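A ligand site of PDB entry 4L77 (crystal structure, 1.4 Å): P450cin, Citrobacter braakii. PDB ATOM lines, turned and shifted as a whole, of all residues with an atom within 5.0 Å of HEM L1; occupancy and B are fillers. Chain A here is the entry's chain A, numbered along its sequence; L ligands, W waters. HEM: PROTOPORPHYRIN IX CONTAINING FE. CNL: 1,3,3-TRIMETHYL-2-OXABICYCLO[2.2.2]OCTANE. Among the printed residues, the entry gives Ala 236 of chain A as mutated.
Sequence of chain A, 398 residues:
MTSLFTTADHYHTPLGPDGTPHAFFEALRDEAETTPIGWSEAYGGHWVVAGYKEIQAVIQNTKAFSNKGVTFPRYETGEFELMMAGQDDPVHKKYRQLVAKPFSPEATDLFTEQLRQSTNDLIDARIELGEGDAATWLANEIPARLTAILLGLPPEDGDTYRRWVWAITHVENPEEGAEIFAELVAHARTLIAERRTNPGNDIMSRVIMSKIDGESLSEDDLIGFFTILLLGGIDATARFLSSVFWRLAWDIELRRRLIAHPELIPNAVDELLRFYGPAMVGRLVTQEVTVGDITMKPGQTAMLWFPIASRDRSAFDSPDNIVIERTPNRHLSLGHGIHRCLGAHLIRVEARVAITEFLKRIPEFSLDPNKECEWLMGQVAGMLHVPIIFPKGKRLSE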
ATOM      1  N   ILE A  59      24.040  15.859  -7.181  1.00  0.00           N
ATOM      2  CA  ILE A  59      23.802  16.963  -8.103  1.00  0.00           C
ATOM      3  C   ILE A  59      22.292  17.131  -8.339  1.00  0.00           C
ATOM      4  O   ILE A  59      21.862  18.208  -8.679  1.00  0.00           O
ATOM      5  CB  ILE A  59      24.646  16.713  -9.408  1.00  0.00           C
ATOM      6  CG1 ILE A  59      25.074  18.030 -10.059  1.00  0.00           C
ATOM      7  CG2 ILE A  59      23.936  15.750 -10.283  1.00  0.00           C
ATOM      8  CD1 ILE A  59      26.094  17.862 -11.217  1.00  0.00           C
ATOM      9  N   ASN A  67      24.618  25.627  -5.025  1.00  0.00           N
ATOM     10  CA  ASN A  67      25.645  26.133  -5.925  1.00  0.00           C
ATOM     11  C   ASN A  67      26.372  27.373  -5.409  1.00  0.00           C
ATOM     12  O   ASN A  67      27.241  27.897  -6.083  1.00  0.00           O
ATOM     13  CB  ASN A  67      25.081  26.368  -7.346  1.00  0.00           C
ATOM     14  CG  ASN A  67      25.261  25.132  -8.170  1.00  0.00           C
ATOM     15  OD1 ASN A  67      24.805  24.041  -7.750  1.00  0.00           O
ATOM     16  ND2 ASN A  67      25.954  25.263  -9.314  1.00  0.00           N
ATOM     17  N   VAL A  70      29.908  26.400  -5.709  1.00  0.00           N
ATOM     18  CA  VAL A  70      30.270  25.848  -7.012  1.00  0.00           C
ATOM     19  C   VAL A  70      31.781  25.872  -7.273  1.00  0.00           C
ATOM     20  O   VAL A  70      32.322  24.955  -7.905  1.00  0.00           O
ATOM     21  CB  VAL A  70      29.507  26.586  -8.186  1.00  0.00           C
ATOM     22  CG1 VAL A  70      29.921  28.073  -8.318  1.00  0.00           C
ATOM     23  CG2 VAL A  70      29.689  25.818  -9.526  1.00  0.00           C
ATOM     24  N   MET A  83      27.423  34.513 -11.809  1.00  0.00           N
ATOM     25  CA  MET A  83      26.110  34.552 -12.377  1.00  0.00           C
ATOM     26  C   MET A  83      25.657  33.166 -12.916  1.00  0.00           C
ATOM     27  O   MET A  83      26.397  32.492 -13.626  1.00  0.00           O
ATOM     28  CB  MET A  83      26.132  35.604 -13.496  1.00  0.00           C
ATOM     29  CG  MET A  83      24.846  35.724 -14.243  1.00  0.00           C
ATOM     30  SD  MET A  83      23.417  36.195 -13.226  1.00  0.00           S
ATOM     31  CE  MET A  83      23.808  37.864 -12.708  1.00  0.00           C
ATOM     32  N   MET A  84      24.446  32.751 -12.546  1.00  0.00           N
ATOM     33  CA  MET A  84      23.850  31.430 -12.836  1.00  0.00           C
ATOM     34  C   MET A  84      24.553  30.297 -12.082  1.00  0.00           C
ATOM     35  O   MET A  84      23.925  29.581 -11.251  1.00  0.00           O
ATOM     36  CB  MET A  84      23.813  31.098 -14.339  1.00  0.00           C
ATOM     37  CG  MET A  84      22.901  32.035 -15.125  1.00  0.00           C
ATOM     38  SD  MET A  84      23.069  31.798 -16.930  1.00  0.00           S
ATOM     39  CE  MET A  84      24.670  32.577 -17.198  1.00  0.00           C
ATOM     40  N   ALA A  85      25.857  30.128 -12.345  1.00  0.00           N
ATOM     41  CA  ALA A  85      26.606  28.987 -11.796  1.00  0.00           C
ATOM     42  C   ALA A  85      26.647  29.021 -10.273  1.00  0.00           C
ATOM     43  O   ALA A  85      26.773  27.967  -9.647  1.00  0.00           O
ATOM     44  CB  ALA A  85      28.022  28.941 -12.359  1.00  0.00           C
ATOM     45  N   HIS A  92      18.353  31.445  -9.798  1.00  0.00           N
ATOM     46  CA  HIS A  92      19.110  30.852 -10.901  1.00  0.00           C
ATOM     47  C   HIS A  92      18.287  30.721 -12.197  1.00  0.00           C
ATOM     48  O   HIS A  92      18.747  31.102 -13.292  1.00  0.00           O
ATOM     49  CB  HIS A  92      19.635  29.481 -10.471  1.00  0.00           C
ATOM     50  CG  HIS A  92      19.962  28.573 -11.622  1.00  0.00           C
ATOM     51  ND1 HIS A  92      19.058  27.651 -12.108  1.00  0.00           N
ATOM     52  CD2 HIS A  92      21.084  28.431 -12.385  1.00  0.00           C
ATOM     53  CE1 HIS A  92      19.589  26.993 -13.127  1.00  0.00           C
ATOM     54  NE2 HIS A  92      20.815  27.449 -13.313  1.00  0.00           N
ATOM     55  N   ARG A  96      19.070  32.474 -15.863  1.00  0.00           N
ATOM     56  CA  ARG A  96      19.436  31.614 -16.998  1.00  0.00           C
ATOM     57  C   ARG A  96      18.435  31.783 -18.159  1.00  0.00           C
ATOM     58  O   ARG A  96      18.826  31.761 -19.330  1.00  0.00           O
ATOM     59  CB  ARG A  96      19.516  30.141 -16.607  1.00  0.00           C
ATOM     60  CG  ARG A  96      19.961  29.257 -17.770  1.00  0.00           C
ATOM     61  CD  ARG A  96      20.269  27.861 -17.323  1.00  0.00           C
ATOM     62  NE  ARG A  96      20.516  27.012 -18.482  1.00  0.00           N
ATOM     63  CZ  ARG A  96      21.386  25.995 -18.535  1.00  0.00           C
ATOM     64  NH1 ARG A  96      22.134  25.672 -17.479  1.00  0.00           N
ATOM     65  NH2 ARG A  96      21.489  25.301 -19.676  1.00  0.00           N
ATOM     66  N   PHE A 103      22.146  30.573 -26.602  1.00  0.00           N
ATOM     67  CA  PHE A 103      22.933  29.359 -26.507  1.00  0.00           C
ATOM     68  C   PHE A 103      22.215  28.109 -27.002  1.00  0.00           C
ATOM     69  O   PHE A 103      22.750  27.041 -26.920  1.00  0.00           O
ATOM     70  CB  PHE A 103      23.408  29.192 -25.060  1.00  0.00           C
ATOM     71  CG  PHE A 103      24.531  30.109 -24.716  1.00  0.00           C
ATOM     72  CD1 PHE A 103      25.839  29.795 -25.137  1.00  0.00           C
ATOM     73  CD2 PHE A 103      24.301  31.311 -24.066  1.00  0.00           C
ATOM     74  CE1 PHE A 103      26.904  30.672 -24.853  1.00  0.00           C
ATOM     75  CE2 PHE A 103      25.372  32.176 -23.792  1.00  0.00           C
ATOM     76  CZ  PHE A 103      26.663  31.846 -24.163  1.00  0.00           C
ATOM     77  N   ILE A 228      30.808  35.563 -16.261  1.00  0.00           N
ATOM     78  CA  ILE A 228      30.604  34.127 -16.337  1.00  0.00           C
ATOM     79  C   ILE A 228      30.672  33.661 -17.810  1.00  0.00           C
ATOM     80  O   ILE A 228      31.152  32.532 -18.127  1.00  0.00           O
ATOM     81  CB  ILE A 228      29.280  33.712 -15.676  1.00  0.00           C
ATOM     82  CG1 ILE A 228      29.294  32.205 -15.378  1.00  0.00           C
ATOM     83  CG2 ILE A 228      28.058  34.079 -16.487  1.00  0.00           C
ATOM     84  CD1 ILE A 228      30.194  31.884 -14.171  1.00  0.00           C
ATOM     85  N   LEU A 229      30.227  34.507 -18.733  1.00  0.00           N
ATOM     86  CA  LEU A 229      30.239  34.099 -20.164  1.00  0.00           C
ATOM     87  C   LEU A 229      31.665  34.121 -20.706  1.00  0.00           C
ATOM     88  O   LEU A 229      32.067  33.307 -21.528  1.00  0.00           O
ATOM     89  CB  LEU A 229      29.343  35.001 -20.996  1.00  0.00           C
ATOM     90  CG  LEU A 229      27.874  34.911 -20.600  1.00  0.00           C
ATOM     91  CD1 LEU A 229      27.048  35.904 -21.421  1.00  0.00           C
ATOM     92  CD2 LEU A 229      27.334  33.435 -20.743  1.00  0.00           C
ATOM     93  N   GLY A 232      33.361  31.100 -18.848  1.00  0.00           N
ATOM     94  CA  GLY A 232      32.898  29.836 -19.388  1.00  0.00           C
ATOM     95  C   GLY A 232      33.328  29.645 -20.827  1.00  0.00           C
ATOM     96  O   GLY A 232      33.718  28.550 -21.219  1.00  0.00           O
ATOM     97  N   GLY A 233      33.261  30.705 -21.616  1.00  0.00           N
ATOM     98  CA  GLY A 233      33.539  30.625 -23.036  1.00  0.00           C
ATOM     99  C   GLY A 233      34.974  30.349 -23.390  1.00  0.00           C
ATOM    100  O   GLY A 233      35.210  29.706 -24.414  1.00  0.00           O
ATOM    101  N   ALA A 236      37.464  26.457 -20.040  1.00  0.00           N
ATOM    102  CA  ALA A 236      37.378  25.003 -20.135  1.00  0.00           C
ATOM    103  C   ALA A 236      37.404  24.569 -21.586  1.00  0.00           C
ATOM    104  O   ALA A 236      37.924  23.511 -21.895  1.00  0.00           O
ATOM    105  CB  ALA A 236      36.119  24.504 -19.444  1.00  0.00           C
ATOM    106  N   THR A 237      36.878  25.407 -22.462  1.00  0.00           N
ATOM    107  CA  THR A 237      36.920  25.085 -23.892  1.00  0.00           C
ATOM    108  C   THR A 237      38.377  24.951 -24.365  1.00  0.00           C
ATOM    109  O   THR A 237      38.755  24.014 -25.052  1.00  0.00           O
ATOM    110  CB  THR A 237      36.243  26.171 -24.671  1.00  0.00           C
ATOM    111  OG1 THR A 237      36.805  27.452 -24.188  1.00  0.00           O
ATOM    112  CG2 THR A 237      34.729  26.115 -24.391  1.00  0.00           C
ATOM    113  N   PHE A 240      40.069  21.811 -22.857  1.00  0.00           N
ATOM    114  CA  PHE A 240      39.549  20.602 -23.507  1.00  0.00           C
ATOM    115  C   PHE A 240      40.159  20.443 -24.885  1.00  0.00           C
ATOM    116  O   PHE A 240      40.716  19.388 -25.215  1.00  0.00           O
ATOM    117  CB  PHE A 240      38.035  20.669 -23.614  1.00  0.00           C
ATOM    118  CG  PHE A 240      37.489  19.533 -24.438  1.00  0.00           C
ATOM    119  CD1 PHE A 240      36.767  19.756 -25.582  1.00  0.00           C
ATOM    120  CD2 PHE A 240      37.667  18.196 -24.004  1.00  0.00           C
ATOM    121  CE1 PHE A 240      36.252  18.704 -26.350  1.00  0.00           C
ATOM    122  CE2 PHE A 240      37.156  17.127 -24.758  1.00  0.00           C
ATOM    123  CZ  PHE A 240      36.442  17.384 -25.929  1.00  0.00           C
ATOM    124  N   LEU A 273      35.067  14.246 -24.530  1.00  0.00           N
ATOM    125  CA  LEU A 273      34.526  14.964 -23.361  1.00  0.00           C
ATOM    126  C   LEU A 273      34.450  14.074 -22.142  1.00  0.00           C
ATOM    127  O   LEU A 273      34.760  14.517 -21.039  1.00  0.00           O
ATOM    128  CB  LEU A 273      33.163  15.571 -23.646  1.00  0.00           C
ATOM    129  CG  LEU A 273      33.199  16.868 -24.437  1.00  0.00           C
ATOM    130  CD1 LEU A 273      31.781  17.205 -24.900  1.00  0.00           C
ATOM    131  CD2 LEU A 273      33.723  18.034 -23.574  1.00  0.00           C
ATOM    132  N   PRO A 278      37.399  18.807 -18.679  1.00  0.00           N
ATOM    133  CA  PRO A 278      38.226  19.586 -17.730  1.00  0.00           C
ATOM    134  C   PRO A 278      37.658  19.815 -16.343  1.00  0.00           C
ATOM    135  O   PRO A 278      38.416  20.132 -15.427  1.00  0.00           O
ATOM    136  CB  PRO A 278      38.363  20.945 -18.420  1.00  0.00           C
ATOM    137  CG  PRO A 278      38.217  20.648 -19.879  1.00  0.00           C
ATOM    138  CD  PRO A 278      37.200  19.521 -19.959  1.00  0.00           C
ATOM    139  N   ALA A 279      36.346  19.753 -16.153  1.00  0.00           N
ATOM    140  CA  ALA A 279      35.689  20.381 -15.008  1.00  0.00           C
ATOM    141  C   ALA A 279      35.408  19.505 -13.823  1.00  0.00           C
ATOM    142  O   ALA A 279      35.118  18.281 -13.928  1.00  0.00           O
ATOM    143  CB  ALA A 279      34.384  21.014 -15.441  1.00  0.00           C
ATOM    144  N   VAL A 281      33.082  20.436 -10.045  1.00  0.00           N
ATOM    145  CA  VAL A 281      32.326  21.514  -9.389  1.00  0.00           C
ATOM    146  C   VAL A 281      32.117  21.152  -7.941  1.00  0.00           C
ATOM    147  O   VAL A 281      32.146  19.989  -7.557  1.00  0.00           O
ATOM    148  CB  VAL A 281      30.944  21.767 -10.037  1.00  0.00           C
ATOM    149  CG1 VAL A 281      31.118  22.228 -11.473  1.00  0.00           C
ATOM    150  CG2 VAL A 281      30.075  20.532  -9.948  1.00  0.00           C
ATOM    151  N   ARG A 283      29.710  21.812  -4.215  1.00  0.00           N
ATOM    152  CA  ARG A 283      28.398  22.096  -3.654  1.00  0.00           C
ATOM    153  C   ARG A 283      28.573  22.413  -2.192  1.00  0.00           C
ATOM    154  O   ARG A 283      29.338  21.716  -1.511  1.00  0.00           O
ATOM    155  CB  ARG A 283      27.439  20.919  -3.785  1.00  0.00           C
ATOM    156  CG  ARG A 283      27.052  20.528  -5.234  1.00  0.00           C
ATOM    157  CD  ARG A 283      26.223  21.567  -5.860  1.00  0.00           C
ATOM    158  NE  ARG A 283      25.730  21.184  -7.186  1.00  0.00           N
ATOM    159  CZ  ARG A 283      26.262  21.569  -8.352  1.00  0.00           C
ATOM    160  NH1 ARG A 283      27.423  22.224  -8.399  1.00  0.00           N
ATOM    161  NH2 ARG A 283      25.657  21.283  -9.491  1.00  0.00           N
ATOM    162  N   PHE A 306      33.969  14.704 -11.340  1.00  0.00           N
ATOM    163  CA  PHE A 306      33.419  14.144 -12.599  1.00  0.00           C
ATOM    164  C   PHE A 306      34.406  13.220 -13.319  1.00  0.00           C
ATOM    165  O   PHE A 306      33.947  12.220 -13.851  1.00  0.00           O
ATOM    166  CB  PHE A 306      33.025  15.284 -13.521  1.00  0.00           C
ATOM    167  CG  PHE A 306      31.867  16.121 -13.051  1.00  0.00           C
ATOM    168  CD1 PHE A 306      31.887  17.472 -13.318  1.00  0.00           C
ATOM    169  CD2 PHE A 306      30.749  15.576 -12.389  1.00  0.00           C
ATOM    170  CE1 PHE A 306      30.819  18.267 -12.938  1.00  0.00           C
ATOM    171  CE2 PHE A 306      29.693  16.379 -12.010  1.00  0.00           C
ATOM    172  CZ  PHE A 306      29.741  17.728 -12.266  1.00  0.00           C
ATOM    173  N   LEU A 332      29.297  12.835 -17.174  1.00  0.00           N
ATOM    174  CA  LEU A 332      28.969  14.006 -16.387  1.00  0.00           C
ATOM    175  C   LEU A 332      29.909  15.199 -16.650  1.00  0.00           C
ATOM    176  O   LEU A 332      29.922  16.171 -15.874  1.00  0.00           O
ATOM    177  CB  LEU A 332      29.012  13.609 -14.907  1.00  0.00           C
ATOM    178  CG  LEU A 332      28.005  12.541 -14.492  1.00  0.00           C
ATOM    179  CD1 LEU A 332      28.269  11.992 -13.085  1.00  0.00           C
ATOM    180  CD2 LEU A 332      26.621  13.122 -14.543  1.00  0.00           C
ATOM    181  N   SER A 333      30.642  15.181 -17.758  1.00  0.00           N
ATOM    182  CA  SER A 333      31.608  16.264 -17.962  1.00  0.00           C
ATOM    183  C   SER A 333      30.959  17.639 -18.164  1.00  0.00           C
ATOM    184  O   SER A 333      31.625  18.647 -17.932  1.00  0.00           O
ATOM    185  CB  SER A 333      32.495  15.943 -19.145  1.00  0.00           C
ATOM    186  OG  SER A 333      33.256  14.796 -18.858  1.00  0.00           O
ATOM    187  N   LEU A 334      29.711  17.682 -18.591  1.00  0.00           N
ATOM    188  CA  LEU A 334      29.001  18.942 -18.786  1.00  0.00           C
ATOM    189  C   LEU A 334      27.974  19.138 -17.670  1.00  0.00           C
ATOM    190  O   LEU A 334      27.079  19.969 -17.793  1.00  0.00           O
ATOM    191  CB  LEU A 334      28.368  18.995 -20.192  1.00  0.00           C
ATOM    192  CG  LEU A 334      29.372  18.935 -21.346  1.00  0.00           C
ATOM    193  CD1 LEU A 334      28.628  18.822 -22.663  1.00  0.00           C
ATOM    194  CD2 LEU A 334      30.249  20.204 -21.341  1.00  0.00           C
ATOM    195  N   GLY A 335      28.087  18.376 -16.570  1.00  0.00           N
ATOM    196  CA  GLY A 335      27.148  18.454 -15.476  1.00  0.00           C
ATOM    197  C   GLY A 335      25.879  17.652 -15.742  1.00  0.00           C
ATOM    198  O   GLY A 335      25.812  16.794 -16.642  1.00  0.00           O
ATOM    199  N   ILE A 338      19.786  20.983 -13.177  1.00  0.00           N
ATOM    200  CA  ILE A 338      19.405  22.363 -13.489  1.00  0.00           C
ATOM    201  C   ILE A 338      20.573  23.275 -13.866  1.00  0.00           C
ATOM    202  O   ILE A 338      20.367  24.311 -14.555  1.00  0.00           O
ATOM    203  CB  ILE A 338      18.615  22.992 -12.342  1.00  0.00           C
ATOM    204  CG1 ILE A 338      19.500  23.208 -11.125  1.00  0.00           C
ATOM    205  CG2 ILE A 338      17.378  22.139 -12.017  1.00  0.00           C
ATOM    206  CD1 ILE A 338      18.880  24.158 -10.095  1.00  0.00           C
ATOM    207  N   HIS A 339      21.826  22.917 -13.488  1.00  0.00           N
ATOM    208  CA  HIS A 339      22.977  23.746 -13.882  1.00  0.00           C
ATOM    209  C   HIS A 339      23.715  23.211 -15.114  1.00  0.00           C
ATOM    210  O   HIS A 339      24.823  23.661 -15.394  1.00  0.00           O
ATOM    211  CB  HIS A 339      23.986  23.852 -12.694  1.00  0.00           C
ATOM    212  CG  HIS A 339      23.415  24.639 -11.554  1.00  0.00           C
ATOM    213  ND1 HIS A 339      23.358  26.008 -11.547  1.00  0.00           N
ATOM    214  CD2 HIS A 339      22.864  24.231 -10.382  1.00  0.00           C
ATOM    215  CE1 HIS A 339      22.810  26.433 -10.420  1.00  0.00           C
ATOM    216  NE2 HIS A 339      22.493  25.359  -9.681  1.00  0.00           N
ATOM    217  N   ARG A 340      23.156  22.237 -15.841  1.00  0.00           N
ATOM    218  CA  ARG A 340      23.886  21.583 -16.923  1.00  0.00           C
ATOM    219  C   ARG A 340      24.406  22.635 -17.876  1.00  0.00           C
ATOM    220  O   ARG A 340      23.712  23.597 -18.216  1.00  0.00           O
ATOM    221  CB  ARG A 340      22.992  20.563 -17.675  1.00  0.00           C
ATOM    222  CG  ARG A 340      23.846  19.619 -18.614  1.00  0.00           C
ATOM    223  CD  ARG A 340      23.039  18.403 -19.185  1.00  0.00           C
ATOM    224  NE  ARG A 340      23.895  17.513 -19.977  1.00  0.00           N
ATOM    225  CZ  ARG A 340      24.164  17.719 -21.261  1.00  0.00           C
ATOM    226  NH1 ARG A 340      23.666  18.792 -21.881  1.00  0.00           N
ATOM    227  NH2 ARG A 340      24.986  16.874 -21.899  1.00  0.00           N
ATOM    228  N   CYS A 341      25.642  22.459 -18.311  1.00  0.00           N
ATOM    229  CA  CYS A 341      26.371  23.449 -19.059  1.00  0.00           C
ATOM    230  C   CYS A 341      25.567  24.224 -20.114  1.00  0.00           C
ATOM    231  O   CYS A 341      25.060  23.656 -21.078  1.00  0.00           O
ATOM    232  CB  CYS A 341      27.528  22.771 -19.747  1.00  0.00           C
ATOM    233  SG  CYS A 341      28.545  23.925 -20.709  1.00  0.00           S
ATOM    234  N   LEU A 342      25.567  25.550 -19.942  1.00  0.00           N
ATOM    235  CA  LEU A 342      24.903  26.434 -20.880  1.00  0.00           C
ATOM    236  C   LEU A 342      25.537  26.355 -22.263  1.00  0.00           C
ATOM    237  O   LEU A 342      24.849  26.449 -23.317  1.00  0.00           O
ATOM    238  CB  LEU A 342      24.959  27.872 -20.311  1.00  0.00           C
ATOM    239  CG  LEU A 342      23.985  28.995 -20.672  1.00  0.00           C
ATOM    240  CD1 LEU A 342      24.667  30.387 -20.673  1.00  0.00           C
ATOM    241  CD2 LEU A 342      22.907  28.736 -21.515  1.00  0.00           C
ATOM    242  N   GLY A 343      26.843  26.152 -22.286  1.00  0.00           N
ATOM    243  CA  GLY A 343      27.598  26.109 -23.540  1.00  0.00           C
ATOM    244  C   GLY A 343      27.708  24.726 -24.181  1.00  0.00           C
ATOM    245  O   GLY A 343      28.566  24.534 -25.028  1.00  0.00           O
ATOM    246  N   LEU A 346      27.516  24.576 -27.967  1.00  0.00           N
ATOM    247  CA  LEU A 346      28.569  25.424 -28.515  1.00  0.00           C
ATOM    248  C   LEU A 346      29.926  24.698 -28.458  1.00  0.00           C
ATOM    249  O   LEU A 346      30.677  24.684 -29.467  1.00  0.00           O
ATOM    250  CB  LEU A 346      28.624  26.742 -27.750  1.00  0.00           C
ATOM    251  CG  LEU A 346      29.647  27.736 -28.271  1.00  0.00           C
ATOM    252  CD1 LEU A 346      29.469  28.039 -29.753  1.00  0.00           C
ATOM    253  CD2 LEU A 346      29.535  29.018 -27.419  1.00  0.00           C
ATOM    254  N   ILE A 347      30.287  24.072 -27.315  1.00  0.00           N
ATOM    255  CA  ILE A 347      31.585  23.397 -27.345  1.00  0.00           C
ATOM    256  C   ILE A 347      31.551  22.216 -28.326  1.00  0.00           C
ATOM    257  O   ILE A 347      32.582  21.903 -28.928  1.00  0.00           O
ATOM    258  CB  ILE A 347      32.061  22.978 -25.941  1.00  0.00           C
ATOM    259  CG1 ILE A 347      33.446  22.296 -25.974  1.00  0.00           C
ATOM    260  CG2 ILE A 347      31.086  22.087 -25.263  1.00  0.00           C
ATOM    261  CD1 ILE A 347      34.573  23.111 -26.623  1.00  0.00           C
HETATM  262  CHA HEM L   1      27.866  25.059 -16.304  1.00  0.00           C
HETATM  263  CHB HEM L   1      31.507  22.340 -17.882  1.00  0.00           C
HETATM  264  CHC HEM L   1      31.955  25.260 -21.745  1.00  0.00           C
HETATM  265  CHD HEM L   1      28.957  28.431 -19.700  1.00  0.00           C
HETATM  266  C1A HEM L   1      28.772  24.047 -16.461  1.00  0.00           C
HETATM  267  C2A HEM L   1      28.799  22.851 -15.595  1.00  0.00           C
HETATM  268  C3A HEM L   1      29.844  22.108 -16.027  1.00  0.00           C
HETATM  269  C4A HEM L   1      30.425  22.770 -17.169  1.00  0.00           C
HETATM  270  CMA HEM L   1      30.315  20.769 -15.410  1.00  0.00           C
HETATM  271  CAA HEM L   1      27.825  22.550 -14.462  1.00  0.00           C
HETATM  272  CBA HEM L   1      28.011  23.437 -13.272  1.00  0.00           C
HETATM  273  CGA HEM L   1      27.435  22.847 -12.005  1.00  0.00           C
HETATM  274  O1A HEM L   1      26.872  21.724 -11.986  1.00  0.00           O
HETATM  275  O2A HEM L   1      27.595  23.510 -10.931  1.00  0.00           O
HETATM  276  C1B HEM L   1      31.926  22.906 -19.050  1.00  0.00           C
HETATM  277  C2B HEM L   1      32.943  22.332 -19.928  1.00  0.00           C
HETATM  278  C3B HEM L   1      33.096  23.155 -21.008  1.00  0.00           C
HETATM  279  C4B HEM L   1      32.143  24.235 -20.828  1.00  0.00           C
HETATM  280  CMB HEM L   1      33.674  21.021 -19.560  1.00  0.00           C
HETATM  281  CAB HEM L   1      33.975  23.023 -22.247  1.00  0.00           C
HETATM  282  CBB HEM L   1      34.770  21.985 -22.466  1.00  0.00           C
HETATM  283  C1C HEM L   1      31.090  26.320 -21.571  1.00  0.00           C
HETATM  284  C2C HEM L   1      30.915  27.424 -22.532  1.00  0.00           C
HETATM  285  C3C HEM L   1      30.087  28.306 -21.947  1.00  0.00           C
HETATM  286  C4C HEM L   1      29.763  27.822 -20.625  1.00  0.00           C
HETATM  287  CMC HEM L   1      31.490  27.435 -23.940  1.00  0.00           C
HETATM  288  CAC HEM L   1      29.553  29.648 -22.458  1.00  0.00           C
HETATM  289  CBC HEM L   1      30.124  30.314 -23.458  1.00  0.00           C
HETATM  290  C1D HEM L   1      28.438  27.824 -18.587  1.00  0.00           C
HETATM  291  C2D HEM L   1      27.527  28.440 -17.661  1.00  0.00           C
HETATM  292  C3D HEM L   1      27.174  27.432 -16.632  1.00  0.00           C
HETATM  293  C4D HEM L   1      27.921  26.250 -17.015  1.00  0.00           C
HETATM  294  CMD HEM L   1      26.974  29.862 -17.673  1.00  0.00           C
HETATM  295  CAD HEM L   1      26.197  27.660 -15.492  1.00  0.00           C
HETATM  296  CBD HEM L   1      24.821  27.149 -15.953  1.00  0.00           C
HETATM  297  CGD HEM L   1      23.814  27.166 -14.836  1.00  0.00           C
HETATM  298  O1D HEM L   1      22.623  26.944 -15.135  1.00  0.00           O
HETATM  299  O2D HEM L   1      24.260  27.414 -13.684  1.00  0.00           O
HETATM  300  NA  HEM L   1      29.773  23.948 -17.434  1.00  0.00           N
HETATM  301  NB  HEM L   1      31.542  24.072 -19.578  1.00  0.00           N
HETATM  302  NC  HEM L   1      30.377  26.605 -20.387  1.00  0.00           N
HETATM  303  ND  HEM L   1      28.701  26.528 -18.137  1.00  0.00           N
HETATM  304 FE   HEM L   1      29.967  25.217 -19.025  1.00  0.00          FE
HETATM  305  C1  CNL L   2      31.912  27.759 -14.834  1.00  0.00           C
HETATM  306  C2  CNL L   2      30.752  26.787 -14.691  1.00  0.00           C
HETATM  307  C3  CNL L   2      30.861  26.008 -13.448  1.00  0.00           C
HETATM  308  C4  CNL L   2      32.144  26.251 -12.723  1.00  0.00           C
HETATM  309  C5  CNL L   2      32.308  27.653 -12.402  1.00  0.00           C
HETATM  310  C6  CNL L   2      32.130  28.570 -13.574  1.00  0.00           C
HETATM  311  C7  CNL L   2      31.713  28.624 -16.034  1.00  0.00           C
HETATM  312  C8  CNL L   2      33.206  25.918 -13.708  1.00  0.00           C
HETATM  313  C9  CNL L   2      33.097  24.468 -14.165  1.00  0.00           C
HETATM  314  C10 CNL L   2      34.543  26.159 -13.098  1.00  0.00           C
HETATM  315  O   CNL L   2      33.034  26.818 -14.987  1.00  0.00           O
HETATM  316  O   HOH W   1      25.158  20.441 -13.551  1.00  0.00           O
HETATM  317  O   HOH W   2      34.339  18.324 -17.627  1.00  0.00           O
HETATM  318  O   HOH W   3      33.356  25.788 -17.481  1.00  0.00           O
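ND2 of Asn 67 is in hydrogen-bond range of O2A of HEM L1 (2.9 Å).
O2D of HEM L1 lies close to N of Ala 85, at 3.4 Å.
A ring nitrogen (ND1) of His 339 is in hydrogen-bond range of an oxygen (O2D) of HEM L1, at 2.7 Å.
The guanidinium group (NH1) of Arg 96 is in salt-bridge range of an oxygen (O1D) of HEM L1 (2.7 Å).
FE of HEM L1 is bound by SG of Cys 341, at 2.6 Å.
The guanidinium group of Arg 283 is in salt-bridge range of an oxygen (O1A) of HEM L1, 2.8 Å away.
O1D of HEM L1 lies within hydrogen-bond range of NE2 of His 92.
The backbone carbonyl oxygen of Leu 273 sits at hydrogen-bond distance from the side-chain hydroxyl of Ser 333.
The side-chain amide nitrogen (ND2) of Asn 67 is in hydrogen-bond range of the backbone carbonyl oxygen (O) of Ala 85 (2.8 Å).
The backbone carbonyl oxygen (O) of Gly 233 is in hydrogen-bond range of the side-chain hydroxyl (OG1) of Thr 237, 2.8 Å away.
OD1 of Asn 67 lies close to NE of Arg 283.
O of Ile 338 lies close to NE2 of His 92.
The backbone NH (N) of Cys 341 lies within hydrogen-bond range of the backbone carbonyl oxygen (O) of Leu 334 (2.9 Å).
A ring nitrogen (NE2) of His 339 sits close to the side-chain amide oxygen (OD1) of Asn 67, at 3.3 Å.
SG of Cys 341 sits close to N of Gly 343 (3.2 Å).
The backbone carbonyl oxygen of Met 84 lies close to an oxygen (O2D) of HEM L1 (3.3 Å).
CG2 of Val 70 touches O2A of HEM L1, at 3.4 Å.
CE1 of Phe 103 touches CBC of HEM L1, 3.5 Å away.
O of Gly 232 touches C2C of HEM L1, 3.3 Å away.
Gly 233 touches HEM L1 (CA to CBC, 3.5 Å).
Ala 236 touches HEM L1 (O to CBB, 3.5 Å).
CG2 of Thr 237 touches CMC of HEM L1, 3.5 Å away.
CB of Phe 240 touches CBB of HEM L1, 3.7 Å away.
Pro 278 touches HEM L1.
CB of Ala 279 touches CHB of HEM L1, at 3.999 Å.
CG1 of Val 281 touches CGA of HEM L1 (3.8 Å).
Phe 306 touches HEM L1 (CE1 to CMA, 3.6 Å).
O of Ser 333 touches CMB of HEM L1, 3.5 Å away.
Leu 334 touches HEM L1.
N of Gly 335 touches CMA of HEM L1, 3.5 Å away.
Ile 338 touches HEM L1 (O to O1D, 3.5 Å).
CB of Leu 342 touches C2D of HEM L1 (3.7 Å).
Gly 343 touches HEM L1 (CA to C3C, 3.7 Å).
Ile 347 touches HEM L1.
Hydrophobic or aromatic side chains that line HEM L1: Val 70, Met 84, Ala 85, His 92, Phe 103, Ala 236, Phe 240, Pro 278, Ala 279, Val 281, Phe 306, Leu 334, His 339, Leu 342 and Ile 347.
Of the 34 residues printed, 26 come within 4 Å of HEM L1.
The nearest printed residue that does not touch HEM L1 is Ile 59 (4.01 Å).
Water W2 lies within hydrogen-bond range of the backbone carbonyl oxygen of Ser 333 (2.8 Å) and the backbone NH of Ala 279 (2.9 Å).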
